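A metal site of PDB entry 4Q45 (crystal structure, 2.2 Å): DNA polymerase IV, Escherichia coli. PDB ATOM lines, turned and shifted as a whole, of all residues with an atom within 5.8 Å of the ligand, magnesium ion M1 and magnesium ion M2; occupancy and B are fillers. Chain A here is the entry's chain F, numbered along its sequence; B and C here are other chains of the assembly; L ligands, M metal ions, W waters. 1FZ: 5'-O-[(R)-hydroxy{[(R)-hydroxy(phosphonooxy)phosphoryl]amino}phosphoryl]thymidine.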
ATOM      1  N   ASP A   9      15.471   2.608  19.120  1.00  0.00           N
ATOM      2  CA  ASP A   9      14.746   2.919  17.899  1.00  0.00           C
ATOM      3  C   ASP A   9      15.329   4.195  17.292  1.00  0.00           C
ATOM      4  O   ASP A   9      15.268   5.257  17.904  1.00  0.00           O
ATOM      5  CB  ASP A   9      13.260   3.120  18.229  1.00  0.00           C
ATOM      6  CG  ASP A   9      12.371   3.216  16.993  1.00  0.00           C
ATOM      7  OD1 ASP A   9      12.802   3.764  15.957  1.00  0.00           O
ATOM      8  OD2 ASP A   9      11.219   2.735  17.068  1.00  0.00           O
ATOM      9  N   MET A  10      15.885   4.092  16.089  1.00  0.00           N
ATOM     10  CA  MET A  10      16.473   5.248  15.408  1.00  0.00           C
ATOM     11  C   MET A  10      15.404   6.262  14.994  1.00  0.00           C
ATOM     12  O   MET A  10      14.289   5.875  14.627  1.00  0.00           O
ATOM     13  CB  MET A  10      17.256   4.796  14.172  1.00  0.00           C
ATOM     14  CG  MET A  10      18.303   3.712  14.440  1.00  0.00           C
ATOM     15  SD  MET A  10      19.691   4.290  15.433  1.00  0.00           S
ATOM     16  CE  MET A  10      20.409   5.463  14.307  1.00  0.00           C
ATOM     17  N   ASP A  11      15.740   7.549  15.056  1.00  0.00           N
ATOM     18  CA  ASP A  11      14.805   8.613  14.691  1.00  0.00           C
ATOM     19  C   ASP A  11      14.746   8.815  13.182  1.00  0.00           C
ATOM     20  O   ASP A  11      15.786   8.888  12.534  1.00  0.00           O
ATOM     21  CB  ASP A  11      15.230   9.937  15.329  1.00  0.00           C
ATOM     22  CG  ASP A  11      15.300   9.883  16.836  1.00  0.00           C
ATOM     23  OD1 ASP A  11      14.410   9.283  17.468  1.00  0.00           O
ATOM     24  OD2 ASP A  11      16.269  10.455  17.402  1.00  0.00           O
ATOM     25  N   CYS A  12      13.541   8.922  12.633  1.00  0.00           N
ATOM     26  CA  CYS A  12      13.315   9.213  11.205  1.00  0.00           C
ATOM     27  C   CYS A  12      14.307   8.472  10.298  1.00  0.00           C
ATOM     28  O   CYS A  12      14.887   9.062   9.395  1.00  0.00           O
ATOM     29  CB  CYS A  12      13.411  10.721  10.944  1.00  0.00           C
ATOM     30  SG  CYS A  12      12.074  11.660  11.700  1.00  0.00           S
ATOM     31  N   PHE A  13      14.454   7.168  10.547  1.00  0.00           N
ATOM     32  CA  PHE A  13      15.635   6.403  10.133  1.00  0.00           C
ATOM     33  C   PHE A  13      16.175   6.679   8.730  1.00  0.00           C
ATOM     34  O   PHE A  13      17.273   7.258   8.587  1.00  0.00           O
ATOM     35  CB  PHE A  13      15.393   4.912  10.330  1.00  0.00           C
ATOM     36  CG  PHE A  13      16.624   4.081  10.127  1.00  0.00           C
ATOM     37  CD1 PHE A  13      17.819   4.442  10.716  1.00  0.00           C
ATOM     38  CD2 PHE A  13      16.582   2.936   9.339  1.00  0.00           C
ATOM     39  CE1 PHE A  13      18.961   3.679  10.527  1.00  0.00           C
ATOM     40  CE2 PHE A  13      17.726   2.164   9.152  1.00  0.00           C
ATOM     41  CZ  PHE A  13      18.910   2.545   9.749  1.00  0.00           C
ATOM     42  N   PHE A  14      15.427   6.277   7.707  1.00  0.00           N
ATOM     43  CA  PHE A  14      15.873   6.445   6.326  1.00  0.00           C
ATOM     44  C   PHE A  14      16.184   7.926   6.072  1.00  0.00           C
ATOM     45  O   PHE A  14      17.260   8.281   5.570  1.00  0.00           O
ATOM     46  CB  PHE A  14      14.814   5.962   5.319  1.00  0.00           C
ATOM     47  CG  PHE A  14      14.555   4.471   5.349  1.00  0.00           C
ATOM     48  CD1 PHE A  14      15.194   3.639   6.248  1.00  0.00           C
ATOM     49  CD2 PHE A  14      13.662   3.909   4.441  1.00  0.00           C
ATOM     50  CE1 PHE A  14      14.944   2.271   6.262  1.00  0.00           C
ATOM     51  CE2 PHE A  14      13.410   2.539   4.445  1.00  0.00           C
ATOM     52  CZ  PHE A  14      14.052   1.722   5.361  1.00  0.00           C
ATOM     53  N   ALA A  15      15.240   8.782   6.442  1.00  0.00           N
ATOM     54  CA  ALA A  15      15.402  10.220   6.270  1.00  0.00           C
ATOM     55  C   ALA A  15      16.628  10.747   7.008  1.00  0.00           C
ATOM     56  O   ALA A  15      17.367  11.569   6.469  1.00  0.00           O
ATOM     57  CB  ALA A  15      14.153  10.960   6.729  1.00  0.00           C
ATOM     58  N   ILE A  42       4.693   6.685   1.010  1.00  0.00           N
ATOM     59  CA  ILE A  42       5.789   7.172   1.824  1.00  0.00           C
ATOM     60  C   ILE A  42       6.344   6.077   2.745  1.00  0.00           C
ATOM     61  O   ILE A  42       5.618   5.520   3.558  1.00  0.00           O
ATOM     62  CB  ILE A  42       5.306   8.371   2.675  1.00  0.00           C
ATOM     63  CG1 ILE A  42       4.733   9.455   1.763  1.00  0.00           C
ATOM     64  CG2 ILE A  42       6.432   8.920   3.550  1.00  0.00           C
ATOM     65  CD1 ILE A  42       5.697   9.911   0.672  1.00  0.00           C
ATOM     66  N   SER A  43       7.633   5.771   2.591  1.00  0.00           N
ATOM     67  CA  SER A  43       8.320   4.893   3.523  1.00  0.00           C
ATOM     68  C   SER A  43       8.519   5.664   4.815  1.00  0.00           C
ATOM     69  O   SER A  43       8.165   5.184   5.898  1.00  0.00           O
ATOM     70  CB  SER A  43       9.674   4.437   2.978  1.00  0.00           C
ATOM     71  OG  SER A  43       9.525   3.409   2.024  1.00  0.00           O
ATOM     72  N   THR A  44       9.066   6.881   4.705  1.00  0.00           N
ATOM     73  CA  THR A  44       9.106   7.779   5.873  1.00  0.00           C
ATOM     74  C   THR A  44       9.389   9.228   5.507  1.00  0.00           C
ATOM     75  O   THR A  44       9.671   9.553   4.358  1.00  0.00           O
ATOM     76  CB  THR A  44      10.109   7.319   6.970  1.00  0.00           C
ATOM     77  OG1 THR A  44       9.794   7.960   8.205  1.00  0.00           O
ATOM     78  CG2 THR A  44      11.537   7.658   6.587  1.00  0.00           C
ATOM     79  N   ALA A  45       9.309  10.105   6.508  1.00  0.00           N
ATOM     80  CA  ALA A  45       9.498  11.534   6.278  1.00  0.00           C
ATOM     81  C   ALA A  45      10.273  12.171   7.431  1.00  0.00           C
ATOM     82  O   ALA A  45      10.216  11.701   8.563  1.00  0.00           O
ATOM     83  CB  ALA A  45       8.161  12.222   6.089  1.00  0.00           C
ATOM     84  N   TYR A  47      11.152  15.525   9.999  1.00  0.00           N
ATOM     85  CA  TYR A  47      10.263  16.393  10.779  1.00  0.00           C
ATOM     86  C   TYR A  47       9.665  17.589  10.012  1.00  0.00           C
ATOM     87  O   TYR A  47       8.475  17.886  10.176  1.00  0.00           O
ATOM     88  CB  TYR A  47      10.924  16.797  12.113  1.00  0.00           C
ATOM     89  CG  TYR A  47      10.883  15.689  13.145  1.00  0.00           C
ATOM     90  CD1 TYR A  47      11.968  14.846  13.335  1.00  0.00           C
ATOM     91  CD2 TYR A  47       9.751  15.480  13.919  1.00  0.00           C
ATOM     92  CE1 TYR A  47      11.916  13.825  14.259  1.00  0.00           C
ATOM     93  CE2 TYR A  47       9.696  14.469  14.841  1.00  0.00           C
ATOM     94  CZ  TYR A  47      10.785  13.643  15.015  1.00  0.00           C
ATOM     95  OH  TYR A  47      10.721  12.631  15.940  1.00  0.00           O
ATOM     96  N   ARG A  50       6.803  15.968   8.267  1.00  0.00           N
ATOM     97  CA  ARG A  50       5.770  15.523   9.200  1.00  0.00           C
ATOM     98  C   ARG A  50       4.939  16.696   9.708  1.00  0.00           C
ATOM     99  O   ARG A  50       3.757  16.535  10.011  1.00  0.00           O
ATOM    100  CB  ARG A  50       6.396  14.774  10.379  1.00  0.00           C
ATOM    101  CG  ARG A  50       7.095  13.482   9.970  1.00  0.00           C
ATOM    102  CD  ARG A  50       7.653  12.712  11.161  1.00  0.00           C
ATOM    103  NE  ARG A  50       8.412  11.556  10.699  1.00  0.00           N
ATOM    104  CZ  ARG A  50       8.933  10.625  11.506  1.00  0.00           C
ATOM    105  NH1 ARG A  50       8.781  10.701  12.818  1.00  0.00           N
ATOM    106  NH2 ARG A  50       9.611   9.616  10.980  1.00  0.00           N
ATOM    107  N   SER A  56       4.388   7.930   7.346  1.00  0.00           N
ATOM    108  CA  SER A  56       4.680   6.632   6.732  1.00  0.00           C
ATOM    109  C   SER A  56       3.384   5.962   6.298  1.00  0.00           C
ATOM    110  O   SER A  56       2.353   6.169   6.929  1.00  0.00           O
ATOM    111  CB  SER A  56       5.417   5.724   7.713  1.00  0.00           C
ATOM    112  OG  SER A  56       6.701   6.227   8.026  1.00  0.00           O
ATOM    113  N   ALA A  57       3.448   5.190   5.218  1.00  0.00           N
ATOM    114  CA  ALA A  57       2.306   4.463   4.676  1.00  0.00           C
ATOM    115  C   ALA A  57       1.254   5.348   4.006  1.00  0.00           C
ATOM    116  O   ALA A  57       0.244   4.849   3.515  1.00  0.00           O
ATOM    117  CB  ALA A  57       1.650   3.551   5.744  1.00  0.00           C
ATOM    118  N   SER A 102      13.973  -5.161  13.193  1.00  0.00           N
ATOM    119  CA  SER A 102      13.991  -4.457  11.929  1.00  0.00           C
ATOM    120  C   SER A 102      15.366  -3.822  11.828  1.00  0.00           C
ATOM    121  O   SER A 102      16.168  -3.945  12.752  1.00  0.00           O
ATOM    122  CB  SER A 102      12.928  -3.351  11.905  1.00  0.00           C
ATOM    123  OG  SER A 102      13.163  -2.404  12.935  1.00  0.00           O
ATOM    124  N   ASP A 104      16.262  -0.718  12.141  1.00  0.00           N
ATOM    125  CA  ASP A 104      16.505   0.408  13.032  1.00  0.00           C
ATOM    126  C   ASP A 104      16.066   0.197  14.488  1.00  0.00           C
ATOM    127  O   ASP A 104      16.134   1.122  15.298  1.00  0.00           O
ATOM    128  CB  ASP A 104      15.812   1.653  12.468  1.00  0.00           C
ATOM    129  CG  ASP A 104      14.374   1.791  12.932  1.00  0.00           C
ATOM    130  OD1 ASP A 104      13.941   2.926  13.243  1.00  0.00           O
ATOM    131  OD2 ASP A 104      13.649   0.766  12.990  1.00  0.00           O
ATOM    132  N   GLU A 105      15.602  -1.005  14.819  1.00  0.00           N
ATOM    133  CA  GLU A 105      15.059  -1.256  16.151  1.00  0.00           C
ATOM    134  C   GLU A 105      15.679  -2.487  16.794  1.00  0.00           C
ATOM    135  O   GLU A 105      16.093  -3.415  16.087  1.00  0.00           O
ATOM    136  CB  GLU A 105      13.540  -1.463  16.103  1.00  0.00           C
ATOM    137  CG  GLU A 105      12.738  -0.207  15.820  1.00  0.00           C
ATOM    138  CD  GLU A 105      11.241  -0.464  15.898  1.00  0.00           C
ATOM    139  OE1 GLU A 105      10.463   0.389  15.434  1.00  0.00           O
ATOM    140  OE2 GLU A 105      10.863  -1.524  16.445  1.00  0.00           O
ATOM    141  N   ASP A 155       9.005   5.395  22.212  1.00  0.00           N
ATOM    142  CA  ASP A 155       8.230   6.323  21.395  1.00  0.00           C
ATOM    143  C   ASP A 155       7.809   7.577  22.161  1.00  0.00           C
ATOM    144  O   ASP A 155       7.392   8.578  21.564  1.00  0.00           O
ATOM    145  CB  ASP A 155       6.957   5.630  20.887  1.00  0.00           C
ATOM    146  CG  ASP A 155       7.112   5.066  19.499  1.00  0.00           C
ATOM    147  OD1 ASP A 155       7.839   5.684  18.679  1.00  0.00           O
ATOM    148  OD2 ASP A 155       6.499   4.026  19.213  1.00  0.00           O
ATOM    149  N   LYS A 158      10.761  10.849  21.788  1.00  0.00           N
ATOM    150  CA  LYS A 158      11.546  11.041  20.571  1.00  0.00           C
ATOM    151  C   LYS A 158      11.255  12.411  19.966  1.00  0.00           C
ATOM    152  O   LYS A 158      10.178  12.972  20.175  1.00  0.00           O
ATOM    153  CB  LYS A 158      11.269   9.911  19.561  1.00  0.00           C
ATOM    154  CG  LYS A 158       9.870   9.934  18.956  1.00  0.00           C
ATOM    155  CD  LYS A 158       9.696   8.789  17.967  1.00  0.00           C
ATOM    156  CE  LYS A 158       8.307   8.816  17.327  1.00  0.00           C
ATOM    157  NZ  LYS A 158       7.203   8.464  18.274  1.00  0.00           N
ATOM    158  P    DA B   4      -0.072   0.056  -2.221  1.00  0.00           P
ATOM    159  OP1  DA B   4      -0.571  -0.279  -3.583  1.00  0.00           O
ATOM    160  OP2  DA B   4      -0.451  -0.802  -1.078  1.00  0.00           O
ATOM    161  O5'  DA B   4       1.526   0.124  -2.260  1.00  0.00           O
ATOM    162  C5'  DA B   4       2.180   0.987  -3.174  1.00  0.00           C
ATOM    163  C4'  DA B   4       3.661   0.662  -3.221  1.00  0.00           C
ATOM    164  O4'  DA B   4       4.285   1.069  -1.975  1.00  0.00           O
ATOM    165  C3'  DA B   4       3.967  -0.817  -3.370  1.00  0.00           C
ATOM    166  O3'  DA B   4       5.144  -0.972  -4.127  1.00  0.00           O
ATOM    167  C2'  DA B   4       4.193  -1.305  -1.929  1.00  0.00           C
ATOM    168  C1'  DA B   4       4.739  -0.058  -1.235  1.00  0.00           C
ATOM    169  N9   DA B   4       4.279   0.105   0.141  1.00  0.00           N
ATOM    170  C8   DA B   4       3.012  -0.113   0.631  1.00  0.00           C
ATOM    171  N7   DA B   4       2.904   0.122   1.918  1.00  0.00           N
ATOM    172  C5   DA B   4       4.173   0.503   2.302  1.00  0.00           C
ATOM    173  C6   DA B   4       4.705   0.881   3.547  1.00  0.00           C
ATOM    174  N6   DA B   4       3.988   0.934   4.677  1.00  0.00           N
ATOM    175  N1   DA B   4       6.015   1.210   3.582  1.00  0.00           N
ATOM    176  C2   DA B   4       6.733   1.157   2.452  1.00  0.00           C
ATOM    177  N3   DA B   4       6.336   0.821   1.225  1.00  0.00           N
ATOM    178  C4   DA B   4       5.035   0.491   1.220  1.00  0.00           C
ATOM    179  P    DG B   5       5.552  -2.429  -4.671  1.00  0.00           P
ATOM    180  OP1  DG B   5       6.253  -2.228  -5.955  1.00  0.00           O
ATOM    181  OP2  DG B   5       4.365  -3.311  -4.580  1.00  0.00           O
ATOM    182  O5'  DG B   5       6.610  -2.958  -3.601  1.00  0.00           O
ATOM    183  C5'  DG B   5       7.799  -2.231  -3.328  1.00  0.00           C
ATOM    184  C4'  DG B   5       8.465  -2.911  -2.158  1.00  0.00           C
ATOM    185  O4'  DG B   5       7.785  -2.534  -0.927  1.00  0.00           O
ATOM    186  C3'  DG B   5       8.410  -4.438  -2.234  1.00  0.00           C
ATOM    187  O3'  DG B   5       9.708  -4.921  -1.900  1.00  0.00           O
ATOM    188  C2'  DG B   5       7.340  -4.795  -1.208  1.00  0.00           C
ATOM    189  C1'  DG B   5       7.547  -3.705  -0.169  1.00  0.00           C
ATOM    190  N9   DG B   5       6.438  -3.455   0.757  1.00  0.00           N
ATOM    191  C8   DG B   5       5.090  -3.654   0.546  1.00  0.00           C
ATOM    192  N7   DG B   5       4.361  -3.333   1.581  1.00  0.00           N
ATOM    193  C5   DG B   5       5.260  -2.885   2.531  1.00  0.00           C
ATOM    194  C6   DG B   5       5.042  -2.405   3.841  1.00  0.00           C
ATOM    195  O6   DG B   5       3.970  -2.264   4.447  1.00  0.00           O
ATOM    196  N1   DG B   5       6.226  -2.048   4.467  1.00  0.00           N
ATOM    197  C2   DG B   5       7.469  -2.160   3.884  1.00  0.00           C
ATOM    198  N2   DG B   5       8.516  -1.783   4.624  1.00  0.00           N
ATOM    199  N3   DG B   5       7.686  -2.611   2.652  1.00  0.00           N
ATOM    200  C4   DG B   5       6.542  -2.948   2.032  1.00  0.00           C
ATOM    201  P    DC C  18       7.159  -1.754  14.987  1.00  0.00           P
ATOM    202  OP1  DC C  18       8.110  -2.186  16.025  1.00  0.00           O
ATOM    203  OP2  DC C  18       6.264  -0.589  15.203  1.00  0.00           O
ATOM    204  O5'  DC C  18       7.970  -1.515  13.633  1.00  0.00           O
ATOM    205  C5'  DC C  18       8.944  -2.462  13.249  1.00  0.00           C
ATOM    206  C4'  DC C  18       9.556  -2.080  11.926  1.00  0.00           C
ATOM    207  O4'  DC C  18       8.633  -2.382  10.855  1.00  0.00           O
ATOM    208  C3'  DC C  18       9.892  -0.597  11.793  1.00  0.00           C
ATOM    209  O3'  DC C  18      11.300  -0.427  11.731  1.00  0.00           O
ATOM    210  C2'  DC C  18       9.220  -0.158  10.490  1.00  0.00           C
ATOM    211  C1'  DC C  18       8.798  -1.450   9.809  1.00  0.00           C
ATOM    212  N1   DC C  18       7.517  -1.352   9.067  1.00  0.00           N
ATOM    213  C2   DC C  18       7.502  -1.510   7.682  1.00  0.00           C
ATOM    214  O2   DC C  18       8.570  -1.730   7.100  1.00  0.00           O
ATOM    215  N3   DC C  18       6.319  -1.413   7.023  1.00  0.00           N
ATOM    216  C4   DC C  18       5.191  -1.185   7.693  1.00  0.00           C
ATOM    217  N4   DC C  18       4.053  -1.109   6.997  1.00  0.00           N
ATOM    218  C5   DC C  18       5.181  -1.016   9.103  1.00  0.00           C
ATOM    219  C6   DC C  18       6.359  -1.105   9.750  1.00  0.00           C
HETATM  220  O2  1FZ L   1       9.281   1.839   4.983  1.00  0.00           O
HETATM  221  O4  1FZ L   1       5.203   1.969   7.017  1.00  0.00           O
HETATM  222  C4  1FZ L   1       6.592   2.090   7.081  1.00  0.00           C
HETATM  223  C5  1FZ L   1       7.220   2.386   8.292  1.00  0.00           C
HETATM  224  C6  1FZ L   1       8.607   2.495   8.306  1.00  0.00           C
HETATM  225  C5M 1FZ L   1       6.404   2.608   9.560  1.00  0.00           C
HETATM  226  N3  1FZ L   1       7.334   1.901   5.973  1.00  0.00           N
HETATM  227  C2  1FZ L   1       8.666   2.017   6.020  1.00  0.00           C
HETATM  228  N1  1FZ L   1       9.305   2.308   7.155  1.00  0.00           N
HETATM  229  C1' 1FZ L   1      10.767   2.422   7.213  1.00  0.00           C
HETATM  230  C2' 1FZ L   1      11.195   3.830   7.217  1.00  0.00           C
HETATM  231  C3' 1FZ L   1      11.519   4.088   8.624  1.00  0.00           C
HETATM  232  O3' 1FZ L   1      12.521   5.065   8.702  1.00  0.00           O
HETATM  233  O4' 1FZ L   1      11.346   1.804   8.366  1.00  0.00           O
HETATM  234  C4' 1FZ L   1      12.018   2.823   9.093  1.00  0.00           C
HETATM  235  C5' 1FZ L   1      11.785   2.702  10.578  1.00  0.00           C
HETATM  236  O5' 1FZ L   1      10.453   2.648  11.027  1.00  0.00           O
HETATM  237  PA  1FZ L   1       9.884   3.588  12.145  1.00  0.00           P
HETATM  238  O1A 1FZ L   1       8.566   2.992  12.499  1.00  0.00           O
HETATM  239  O2A 1FZ L   1      10.806   3.609  13.404  1.00  0.00           O
HETATM  240  N3A 1FZ L   1       9.636   5.149  11.560  1.00  0.00           N
HETATM  241  PB  1FZ L   1      10.908   6.160  11.678  1.00  0.00           P
HETATM  242  O1B 1FZ L   1      12.063   5.480  12.328  1.00  0.00           O
HETATM  243  O2B 1FZ L   1      11.300   6.620  10.249  1.00  0.00           O
HETATM  244  O3B 1FZ L   1      10.494   7.468  12.491  1.00  0.00           O
HETATM  245  PG  1FZ L   1      10.450   7.506  14.086  1.00  0.00           P
HETATM  246  O1G 1FZ L   1      10.963   6.181  14.644  1.00  0.00           O
HETATM  247  O3G 1FZ L   1       9.026   7.748  14.538  1.00  0.00           O
HETATM  248  O2G 1FZ L   1      11.308   8.631  14.565  1.00  0.00           O
HETATM  249 MG    MG M   1      12.482   4.507  14.168  1.00  0.00          MG
HETATM  250 MG    MG M   2      11.792   1.258  13.951  1.00  0.00          MG
HETATM  251  O   HOH W   1       3.271   2.189   8.674  1.00  0.00           O
HETATM  252  O   HOH W   2       6.257   0.657  13.138  1.00  0.00           O
HETATM  253  O   HOH W   3      11.915  10.517  16.015  1.00  0.00           O
HETATM  254  O   HOH W   4      12.532   6.820  17.221  1.00  0.00           O
HETATM  255  O   HOH W   5       7.289   6.047  10.604  1.00  0.00           O
HETATM  256  O   HOH W   6       6.509   4.067  13.441  1.00  0.00           O
HETATM  257  O   HOH W   7      10.670   1.364   2.573  1.00  0.00           O
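An oxygen (O2B) of the ligand is in hydrogen-bond range of the side-chain hydroxyl (OG1) of Thr 44, 2.9 Å away. An oxygen (O3G) of the ligand is in salt-bridge range of the guanidinium group of Arg 50, at 3.4 Å. N of Phe 14 lies within hydrogen-bond range of O3' of the ligand. O2G of the ligand lies within hydrogen-bond range of N of Cys 12, at 3.0 Å. A nitrogen (N3) of the ligand lies close to the backbone carbonyl oxygen (O) of Ser 43, 3.4 Å away. OG of Ser 43 sits close to O2 of the ligand, at 3.4 Å. The backbone NH (N) of Phe 13 is in hydrogen-bond range of an oxygen (O2B) of the ligand. N1 of DA 4 of chain B lies within hydrogen-bond range of a nitrogen (N3) of the ligand.
Magnesium ion M1 is bound by the side-chain carboxylate (OD1) of Asp 9, 2.0 Å away. An oxygen (O2A) of the ligand binds magnesium ion M1, 2.0 Å away. An oxygen (O1B) of the ligand is bound to magnesium ion M1, at 2.1 Å. O1G of the ligand is bound to magnesium ion M1 (2.3 Å). The backbone carbonyl oxygen (O) of Met 10 is bound to magnesium ion M1, at 2.3 Å. The side-chain carboxylate (OD1) of Asp 104 is bound to magnesium ion M1. Magnesium ion M1 has six donor atoms within binding distance.
Of the 23 residues printed, 4 come within 4 Å of magnesium ion M2. Along chain A the residues within 4 Å of magnesium ion M2 span positions 9 to 105. The nearest printed residue that does not touch magnesium ion M2 is Ser 102 (4.04 Å).
Within 4 Å of magnesium ion M1: Asp 9, Met 10 and Asp 104.
Water W3 lies within hydrogen-bond range of OH of Tyr 47 (2.4 Å), O2G of the ligand (2.5 Å) and OD1 of Asp 11 (3.1 Å). Water W5 bridges the side-chain hydroxyl (OG) of Ser 56 and a nitrogen (N3A) of the ligand. Water W7 lies within hydrogen-bond range of the side-chain hydroxyl of Ser 43 (2.4 Å) and an oxygen (O2) of the ligand (2.8 Å). Water W4 lies within hydrogen-bond range of OD1 of Asp 11, O of Asp 9 and O2G of the ligand. Water W2 bridges OP2 of DC 18 of chain C (2.4 Å) and an oxygen (O1A) of the ligand (3.3 Å).
The side-chain hydroxyl (OG) of Ser 102 sits close to the side-chain carboxylate (OD2) of Asp 104, 3.2 Å away. O3' of DC 18 of chain C is in hydrogen-bond range of OG of Ser 102. SG of Cys 12 lies within hydrogen-bond range of O of Ala 45 (3.6 Å). The backbone carbonyl oxygen of Ala 45 is in hydrogen-bond range of the guanidinium group of Arg 50 (2.8 Å). N of Glu 105 sits close to OG of Ser 102, 3.4 Å away. O of Ser 43 sits at hydrogen-bond distance from OG of Ser 56. N2 of DG 5 of chain B sits close to O2 of DC 18 of chain C (2.5 Å). The side-chain amino group (NZ) of Lys 158 is in salt-bridge range of the side-chain carboxylate (OD1) of Asp 155, 2.9 Å away.
Asp 11 touches the ligand (CA to O2G, 3.5 Å). CB of Ser 56 touches C5M of the ligand, at 3.8 Å. Lys 158 touches the ligand (CE to O3G, 3.1 Å). DG 5 of chain B touches the ligand (N2 to O2, 3.7 Å). Of the 23 residues printed, 16 come within 4 Å of the ligand. The nearest printed residue that does not touch the ligand is Ala 57 (4.1 Å).
Magnesium ion M2 is bound by the side-chain carboxylate (OD2) of Asp 104 (2.1 Å) and the side-chain carboxylate (OE1) of Glu 105 (2.2 Å). Magnesium ion M2 has two donor atoms within binding distance. Slightly farther from magnesium ion M2 lies O2A of the ligand (2.6 Å). Slightly farther from magnesium ion M2 lies the side-chain carboxylate (OD1) of Asp 104 (2.8 Å). Slightly farther from magnesium ion M2 lies O3' of DC 18 of chain C (2.8 Å).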
